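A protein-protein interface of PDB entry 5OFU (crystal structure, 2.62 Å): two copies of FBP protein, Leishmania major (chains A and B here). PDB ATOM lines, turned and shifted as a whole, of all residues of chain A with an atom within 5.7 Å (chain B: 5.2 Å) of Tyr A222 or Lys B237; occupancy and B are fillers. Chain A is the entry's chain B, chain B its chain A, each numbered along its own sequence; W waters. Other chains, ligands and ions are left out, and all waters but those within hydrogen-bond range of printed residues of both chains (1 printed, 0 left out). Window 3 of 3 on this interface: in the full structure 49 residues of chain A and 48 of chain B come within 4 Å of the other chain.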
ATOM      1  N   ASN A 218       9.222  32.055 -26.734  1.00  0.00           N
ATOM      2  CA  ASN A 218       9.670  31.884 -25.342  1.00  0.00           C
ATOM      3  C   ASN A 218      10.876  30.918 -25.235  1.00  0.00           C
ATOM      4  O   ASN A 218      10.698  29.702 -25.159  1.00  0.00           O
ATOM      5  CB  ASN A 218       8.521  31.380 -24.454  1.00  0.00           C
ATOM      6  CG  ASN A 218       8.881  31.371 -22.971  1.00  0.00           C
ATOM      7  OD1 ASN A 218      10.045  31.503 -22.580  1.00  0.00           O
ATOM      8  ND2 ASN A 218       7.873  31.238 -22.132  1.00  0.00           N
ATOM      9  N   GLU A 219      12.086  31.482 -25.159  1.00  0.00           N
ATOM     10  CA  GLU A 219      13.317  30.683 -25.062  1.00  0.00           C
ATOM     11  C   GLU A 219      13.542  30.048 -23.700  1.00  0.00           C
ATOM     12  O   GLU A 219      14.445  29.230 -23.553  1.00  0.00           O
ATOM     13  CB  GLU A 219      14.549  31.495 -25.459  1.00  0.00           C
ATOM     14  CG  GLU A 219      14.563  31.856 -26.937  1.00  0.00           C
ATOM     15  CD  GLU A 219      15.939  32.194 -27.459  1.00  0.00           C
ATOM     16  OE1 GLU A 219      16.859  31.366 -27.270  1.00  0.00           O
ATOM     17  OE2 GLU A 219      16.103  33.286 -28.045  1.00  0.00           O
ATOM     18  N   GLY A 220      12.713  30.378 -22.717  1.00  0.00           N
ATOM     19  CA  GLY A 220      12.653  29.594 -21.484  1.00  0.00           C
ATOM     20  C   GLY A 220      12.377  28.109 -21.683  1.00  0.00           C
ATOM     21  O   GLY A 220      12.733  27.301 -20.842  1.00  0.00           O
ATOM     22  N   ASN A 221      11.727  27.756 -22.790  1.00  0.00           N
ATOM     23  CA  ASN A 221      11.435  26.363 -23.144  1.00  0.00           C
ATOM     24  C   ASN A 221      12.441  25.726 -24.106  1.00  0.00           C
ATOM     25  O   ASN A 221      12.146  24.683 -24.690  1.00  0.00           O
ATOM     26  CB  ASN A 221      10.033  26.307 -23.781  1.00  0.00           C
ATOM     27  CG  ASN A 221       8.971  26.803 -22.847  1.00  0.00           C
ATOM     28  OD1 ASN A 221       9.049  26.615 -21.636  1.00  0.00           O
ATOM     29  ND2 ASN A 221       7.973  27.445 -23.399  1.00  0.00           N
ATOM     30  N   TYR A 222      13.615  26.333 -24.267  1.00  0.00           N
ATOM     31  CA  TYR A 222      14.624  25.851 -25.221  1.00  0.00           C
ATOM     32  C   TYR A 222      14.945  24.368 -25.045  1.00  0.00           C
ATOM     33  O   TYR A 222      14.889  23.606 -26.006  1.00  0.00           O
ATOM     34  CB  TYR A 222      15.901  26.649 -25.062  1.00  0.00           C
ATOM     35  CG  TYR A 222      16.959  26.347 -26.065  1.00  0.00           C
ATOM     36  CD1 TYR A 222      17.886  25.321 -25.853  1.00  0.00           C
ATOM     37  CD2 TYR A 222      17.081  27.126 -27.210  1.00  0.00           C
ATOM     38  CE1 TYR A 222      18.887  25.066 -26.774  1.00  0.00           C
ATOM     39  CE2 TYR A 222      18.085  26.881 -28.133  1.00  0.00           C
ATOM     40  CZ  TYR A 222      18.983  25.851 -27.906  1.00  0.00           C
ATOM     41  OH  TYR A 222      19.972  25.588 -28.815  1.00  0.00           O
ATOM     42  N   GLY A 223      15.262  23.985 -23.814  1.00  0.00           N
ATOM     43  CA  GLY A 223      15.582  22.618 -23.463  1.00  0.00           C
ATOM     44  C   GLY A 223      14.559  21.554 -23.804  1.00  0.00           C
ATOM     45  O   GLY A 223      14.922  20.396 -23.963  1.00  0.00           O
ATOM     46  N   LYS A 224      13.292  21.932 -23.919  1.00  0.00           N
ATOM     47  CA  LYS A 224      12.217  20.987 -24.249  1.00  0.00           C
ATOM     48  C   LYS A 224      11.820  20.966 -25.726  1.00  0.00           C
ATOM     49  O   LYS A 224      10.892  20.238 -26.092  1.00  0.00           O
ATOM     50  CB  LYS A 224      10.993  21.281 -23.375  1.00  0.00           C
ATOM     51  CG  LYS A 224      11.221  20.987 -21.901  1.00  0.00           C
ATOM     52  CD  LYS A 224      10.034  21.436 -21.063  1.00  0.00           C
ATOM     53  CE  LYS A 224      10.044  22.943 -20.828  1.00  0.00           C
ATOM     54  NZ  LYS A 224       8.886  23.400 -20.007  1.00  0.00           N
ATOM     55  N   TRP A 225      12.501  21.741 -26.568  1.00  0.00           N
ATOM     56  CA  TRP A 225      12.163  21.809 -27.996  1.00  0.00           C
ATOM     57  C   TRP A 225      12.746  20.677 -28.810  1.00  0.00           C
ATOM     58  O   TRP A 225      13.690  20.013 -28.391  1.00  0.00           O
ATOM     59  CB  TRP A 225      12.640  23.128 -28.615  1.00  0.00           C
ATOM     60  CG  TRP A 225      11.888  24.341 -28.156  1.00  0.00           C
ATOM     61  CD1 TRP A 225      10.620  24.387 -27.638  1.00  0.00           C
ATOM     62  CD2 TRP A 225      12.345  25.701 -28.209  1.00  0.00           C
ATOM     63  NE1 TRP A 225      10.290  25.671 -27.343  1.00  0.00           N
ATOM     64  CE2 TRP A 225      11.318  26.501 -27.702  1.00  0.00           C
ATOM     65  CE3 TRP A 225      13.525  26.316 -28.650  1.00  0.00           C
ATOM     66  CZ2 TRP A 225      11.423  27.882 -27.622  1.00  0.00           C
ATOM     67  CZ3 TRP A 225      13.630  27.699 -28.562  1.00  0.00           C
ATOM     68  CH2 TRP A 225      12.595  28.459 -28.044  1.00  0.00           C
ATOM     69  N   LYS A 230      15.659  23.981 -32.182  1.00  0.00           N
ATOM     70  CA  LYS A 230      16.876  24.419 -31.493  1.00  0.00           C
ATOM     71  C   LYS A 230      17.937  24.897 -32.478  1.00  0.00           C
ATOM     72  O   LYS A 230      18.583  25.914 -32.237  1.00  0.00           O
ATOM     73  CB  LYS A 230      17.454  23.305 -30.634  1.00  0.00           C
ATOM     74  CG  LYS A 230      16.665  23.001 -29.389  1.00  0.00           C
ATOM     75  CD  LYS A 230      17.393  21.928 -28.605  1.00  0.00           C
ATOM     76  CE  LYS A 230      16.668  21.567 -27.336  1.00  0.00           C
ATOM     77  NZ  LYS A 230      17.043  20.210 -26.862  1.00  0.00           N
ATOM     78  N   GLU A 231      18.101  24.169 -33.584  1.00  0.00           N
ATOM     79  CA  GLU A 231      19.072  24.536 -34.618  1.00  0.00           C
ATOM     80  C   GLU A 231      18.694  25.851 -35.281  1.00  0.00           C
ATOM     81  O   GLU A 231      19.556  26.709 -35.475  1.00  0.00           O
ATOM     82  CB  GLU A 231      19.201  23.443 -35.682  1.00  0.00           C
ATOM     83  CG  GLU A 231      19.954  22.207 -35.230  1.00  0.00           C
ATOM     84  CD  GLU A 231      19.712  21.003 -36.142  1.00  0.00           C
ATOM     85  OE1 GLU A 231      19.569  21.185 -37.380  1.00  0.00           O
ATOM     86  OE2 GLU A 231      19.650  19.870 -35.609  1.00  0.00           O
ATOM     87  N   ILE A 233      16.905  28.318 -34.001  1.00  0.00           N
ATOM     88  CA  ILE A 233      17.126  29.419 -33.068  1.00  0.00           C
ATOM     89  C   ILE A 233      18.606  29.745 -32.920  1.00  0.00           C
ATOM     90  O   ILE A 233      18.984  30.914 -32.894  1.00  0.00           O
ATOM     91  CB  ILE A 233      16.454  29.131 -31.697  1.00  0.00           C
ATOM     92  CG1 ILE A 233      14.915  29.112 -31.841  1.00  0.00           C
ATOM     93  CG2 ILE A 233      16.867  30.145 -30.639  1.00  0.00           C
ATOM     94  CD1 ILE A 233      14.291  30.352 -32.457  1.00  0.00           C
ATOM     95  N   ASP A 234      19.439  28.711 -32.848  1.00  0.00           N
ATOM     96  CA  ASP A 234      20.894  28.905 -32.808  1.00  0.00           C
ATOM     97  C   ASP A 234      21.428  29.583 -34.063  1.00  0.00           C
ATOM     98  O   ASP A 234      22.315  30.427 -33.978  1.00  0.00           O
ATOM     99  CB  ASP A 234      21.623  27.574 -32.613  1.00  0.00           C
ATOM    100  CG  ASP A 234      21.404  26.972 -31.233  1.00  0.00           C
ATOM    101  OD1 ASP A 234      20.811  27.640 -30.340  1.00  0.00           O
ATOM    102  OD2 ASP A 234      21.833  25.813 -31.046  1.00  0.00           O
ATOM    103  N   LYS A 237      20.885  33.300 -33.883  1.00  0.00           N
ATOM    104  CA  LYS A 237      21.893  33.929 -33.026  1.00  0.00           C
ATOM    105  C   LYS A 237      23.318  33.896 -33.576  1.00  0.00           C
ATOM    106  O   LYS A 237      24.006  34.913 -33.551  1.00  0.00           O
ATOM    107  CB  LYS A 237      21.912  33.267 -31.661  1.00  0.00           C
ATOM    108  CG  LYS A 237      20.609  33.396 -30.915  1.00  0.00           C
ATOM    109  CD  LYS A 237      20.596  32.466 -29.731  1.00  0.00           C
ATOM    110  CE  LYS A 237      19.257  32.503 -29.037  1.00  0.00           C
ATOM    111  NZ  LYS A 237      19.372  31.777 -27.748  1.00  0.00           N
ATOM    112  N   TYR B 215      13.091  35.760 -16.735  1.00  0.00           N
ATOM    113  CA  TYR B 215      14.239  36.545 -17.164  1.00  0.00           C
ATOM    114  C   TYR B 215      13.942  37.330 -18.436  1.00  0.00           C
ATOM    115  O   TYR B 215      13.210  36.869 -19.322  1.00  0.00           O
ATOM    116  CB  TYR B 215      15.494  35.675 -17.326  1.00  0.00           C
ATOM    117  CG  TYR B 215      15.523  34.797 -18.549  1.00  0.00           C
ATOM    118  CD1 TYR B 215      14.825  33.602 -18.574  1.00  0.00           C
ATOM    119  CD2 TYR B 215      16.270  35.150 -19.672  1.00  0.00           C
ATOM    120  CE1 TYR B 215      14.855  32.781 -19.683  1.00  0.00           C
ATOM    121  CE2 TYR B 215      16.307  34.336 -20.792  1.00  0.00           C
ATOM    122  CZ  TYR B 215      15.598  33.146 -20.793  1.00  0.00           C
ATOM    123  OH  TYR B 215      15.611  32.295 -21.899  1.00  0.00           O
ATOM    124  N   GLU B 219      17.994  37.987 -26.476  1.00  0.00           N
ATOM    125  CA  GLU B 219      18.831  36.835 -26.885  1.00  0.00           C
ATOM    126  C   GLU B 219      19.262  36.864 -28.343  1.00  0.00           C
ATOM    127  O   GLU B 219      20.066  36.045 -28.749  1.00  0.00           O
ATOM    128  CB  GLU B 219      18.145  35.497 -26.567  1.00  0.00           C
ATOM    129  CG  GLU B 219      18.013  35.247 -25.077  1.00  0.00           C
ATOM    130  CD  GLU B 219      17.815  33.789 -24.741  1.00  0.00           C
ATOM    131  OE1 GLU B 219      18.664  32.966 -25.158  1.00  0.00           O
ATOM    132  OE2 GLU B 219      16.857  33.468 -24.006  1.00  0.00           O
ATOM    133  N   ILE B 233      22.763  32.235 -19.028  1.00  0.00           N
ATOM    134  CA  ILE B 233      21.533  32.056 -19.821  1.00  0.00           C
ATOM    135  C   ILE B 233      21.271  30.578 -20.136  1.00  0.00           C
ATOM    136  O   ILE B 233      20.134  30.121 -20.035  1.00  0.00           O
ATOM    137  CB  ILE B 233      21.560  32.923 -21.108  1.00  0.00           C
ATOM    138  CG1 ILE B 233      21.528  34.418 -20.744  1.00  0.00           C
ATOM    139  CG2 ILE B 233      20.407  32.584 -22.051  1.00  0.00           C
ATOM    140  CD1 ILE B 233      20.381  34.855 -19.857  1.00  0.00           C
ATOM    141  N   ASP B 234      22.321  29.839 -20.480  1.00  0.00           N
ATOM    142  CA  ASP B 234      22.195  28.398 -20.697  1.00  0.00           C
ATOM    143  C   ASP B 234      21.753  27.656 -19.439  1.00  0.00           C
ATOM    144  O   ASP B 234      20.956  26.715 -19.529  1.00  0.00           O
ATOM    145  CB  ASP B 234      23.504  27.796 -21.206  1.00  0.00           C
ATOM    146  CG  ASP B 234      23.860  28.245 -22.618  1.00  0.00           C
ATOM    147  OD1 ASP B 234      23.039  28.906 -23.301  1.00  0.00           O
ATOM    148  OD2 ASP B 234      25.000  27.928 -23.037  1.00  0.00           O
ATOM    149  N   TYR B 235      22.267  28.061 -18.281  1.00  0.00           N
ATOM    150  CA  TYR B 235      21.845  27.443 -17.026  1.00  0.00           C
ATOM    151  C   TYR B 235      20.350  27.655 -16.793  1.00  0.00           C
ATOM    152  O   TYR B 235      19.647  26.726 -16.402  1.00  0.00           O
ATOM    153  CB  TYR B 235      22.654  27.963 -15.840  1.00  0.00           C
ATOM    154  CG  TYR B 235      22.157  27.434 -14.517  1.00  0.00           C
ATOM    155  CD1 TYR B 235      22.551  26.176 -14.054  1.00  0.00           C
ATOM    156  CD2 TYR B 235      21.275  28.183 -13.730  1.00  0.00           C
ATOM    157  CE1 TYR B 235      22.086  25.679 -12.846  1.00  0.00           C
ATOM    158  CE2 TYR B 235      20.803  27.692 -12.523  1.00  0.00           C
ATOM    159  CZ  TYR B 235      21.209  26.435 -12.092  1.00  0.00           C
ATOM    160  OH  TYR B 235      20.745  25.957 -10.896  1.00  0.00           O
ATOM    161  N   LEU B 236      19.861  28.869 -17.057  1.00  0.00           N
ATOM    162  CA  LEU B 236      18.433  29.170 -16.912  1.00  0.00           C
ATOM    163  C   LEU B 236      17.591  28.226 -17.759  1.00  0.00           C
ATOM    164  O   LEU B 236      16.554  27.758 -17.308  1.00  0.00           O
ATOM    165  CB  LEU B 236      18.117  30.631 -17.266  1.00  0.00           C
ATOM    166  CG  LEU B 236      18.797  31.746 -16.456  1.00  0.00           C
ATOM    167  CD1 LEU B 236      18.329  33.102 -16.966  1.00  0.00           C
ATOM    168  CD2 LEU B 236      18.540  31.608 -14.966  1.00  0.00           C
ATOM    169  N   LYS B 237      18.053  27.926 -18.967  1.00  0.00           N
ATOM    170  CA  LYS B 237      17.334  27.007 -19.863  1.00  0.00           C
ATOM    171  C   LYS B 237      17.518  25.522 -19.541  1.00  0.00           C
ATOM    172  O   LYS B 237      16.549  24.777 -19.516  1.00  0.00           O
ATOM    173  CB  LYS B 237      17.765  27.233 -21.302  1.00  0.00           C
ATOM    174  CG  LYS B 237      17.455  28.619 -21.821  1.00  0.00           C
ATOM    175  CD  LYS B 237      18.187  28.862 -23.117  1.00  0.00           C
ATOM    176  CE  LYS B 237      17.968  30.277 -23.599  1.00  0.00           C
ATOM    177  NZ  LYS B 237      18.478  30.391 -24.989  1.00  0.00           N
ATOM    178  N   MET B 238      18.760  25.100 -19.306  1.00  0.00           N
ATOM    179  CA  MET B 238      19.097  23.669 -19.222  1.00  0.00           C
ATOM    180  C   MET B 238      19.048  23.043 -17.822  1.00  0.00           C
ATOM    181  O   MET B 238      18.915  21.827 -17.731  1.00  0.00           O
ATOM    182  CB  MET B 238      20.480  23.410 -19.831  1.00  0.00           C
ATOM    183  CG  MET B 238      20.703  23.947 -21.240  1.00  0.00           C
ATOM    184  SD  MET B 238      19.446  23.454 -22.426  1.00  0.00           S
ATOM    185  CE  MET B 238      20.034  21.799 -22.760  1.00  0.00           C
ATOM    186  N   ASN B 239      19.138  23.834 -16.746  1.00  0.00           N
ATOM    187  CA  ASN B 239      19.191  23.263 -15.387  1.00  0.00           C
ATOM    188  C   ASN B 239      17.963  22.427 -15.077  1.00  0.00           C
ATOM    189  O   ASN B 239      16.891  22.635 -15.657  1.00  0.00           O
ATOM    190  CB  ASN B 239      19.344  24.334 -14.301  1.00  0.00           C
ATOM    191  CG  ASN B 239      18.020  24.953 -13.898  1.00  0.00           C
ATOM    192  OD1 ASN B 239      17.454  24.620 -12.857  1.00  0.00           O
ATOM    193  ND2 ASN B 239      17.492  25.825 -14.749  1.00  0.00           N
ATOM    194  N   ARG B 243      12.408  25.652 -13.884  1.00  0.00           N
ATOM    195  CA  ARG B 243      12.013  26.120 -15.221  1.00  0.00           C
ATOM    196  C   ARG B 243      11.784  27.640 -15.218  1.00  0.00           C
ATOM    197  O   ARG B 243      11.026  28.155 -14.391  1.00  0.00           O
ATOM    198  CB  ARG B 243      10.743  25.412 -15.709  1.00  0.00           C
ATOM    199  CG  ARG B 243      10.822  23.889 -15.763  1.00  0.00           C
ATOM    200  CD  ARG B 243      11.464  23.338 -17.042  1.00  0.00           C
ATOM    201  NE  ARG B 243      12.814  23.860 -17.280  1.00  0.00           N
ATOM    202  CZ  ARG B 243      13.913  23.508 -16.611  1.00  0.00           C
ATOM    203  NH1 ARG B 243      13.869  22.606 -15.631  1.00  0.00           N
ATOM    204  NH2 ARG B 243      15.080  24.077 -16.922  1.00  0.00           N
HETATM  205  O   HOH W   1      13.907  27.290 -18.169  1.00  0.00           O
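The side-chain amino group of Lys A237 lies within salt-bridge range of the side-chain carboxylate of Glu B219 (2.9 Å). The side-chain amino group (NZ) of Lys B237 is in salt-bridge range of the side-chain carboxylate (OE1) of Glu A219 (3.0 Å). OE1 of Glu B219 lies close to OE1 of Glu A219. NZ of Lys A237 sits close to NZ of Lys B237 (3.2 Å).
OE2 of Glu B219 is in hydrogen-bond range of OH of Tyr B215 (2.7 Å). NZ of Lys B237 lies within salt-bridge range of OE1 of Glu B219. The backbone carbonyl oxygen (O) of Lys B237 lies within hydrogen-bond range of the guanidinium group (NH2) of Arg B243, 3.1 Å away. O of Asn B239 is in hydrogen-bond range of NH2 of Arg B243 (2.6 Å). The side-chain carboxylate (OE1) of Glu A219 is in salt-bridge range of the side-chain amino group (NZ) of Lys A237 (2.6 Å). The side-chain hydroxyl of Tyr A222 lies within hydrogen-bond range of the side-chain carboxylate of Asp A234 (2.7 Å).
Of the 10 printed residues of chain B, 4 touch a printed residue of chain A. Hydrophobic or aromatic side chains of chain B that line the printed part of chain A: Tyr B215. Of the 13 printed residues of chain A, 5 touch a printed residue of chain B. Hydrophobic or aromatic side chains of chain A that line the printed part of chain B: Tyr A222. Among the printed residues, Asp or Glu carboxylates within 4 Å of a Lys or Arg side-chain nitrogen of the other chain: Glu A219 with Lys B237 (3.0 Å) and Lys A237 with Glu B219 (2.9 Å).
Glu B219 touches its own counterpart, Glu A219. Glu A219 touches Lys B237, and with the chains exchanged Lys A237 touches Glu B219. Lys A237 touches its own counterpart, Lys B237. Of the 8 pairs that touch across the chains among the printed residues, 4 have their exchanged pair printed and touching as well.
Water W1 bridges O of Leu B236 (2.8 Å) and O of Gly A220 (2.9 Å).
Among the printed residues, merely in contact across the chains: Glu A219 with Tyr B215 (3.5 Å), Gly A220 with Tyr B215 (3.6 Å), Tyr A222 with Lys B237 (3.7 Å) and Lys A224 with Arg B243 (3.9 Å).
Tyr A222 touches just one residue of chain B: Lys B237. Lys B237 touches just these residues of chain A: Glu A219, Tyr A222 and Lys A237. Of the printed residues of chain B, Gly A220 touches Tyr B215. Printed residues of chain B within 4 Å of Lys A237: Glu B219 and Lys B237. Of the printed residues of chain B, Lys A224 touches Arg B243. The nearest residue of chain B that does not touch Tyr A222 is Met B238 (4.2 Å). The nearest residue of chain A that does not touch Lys B237 is Gly A223 (4.6 Å).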
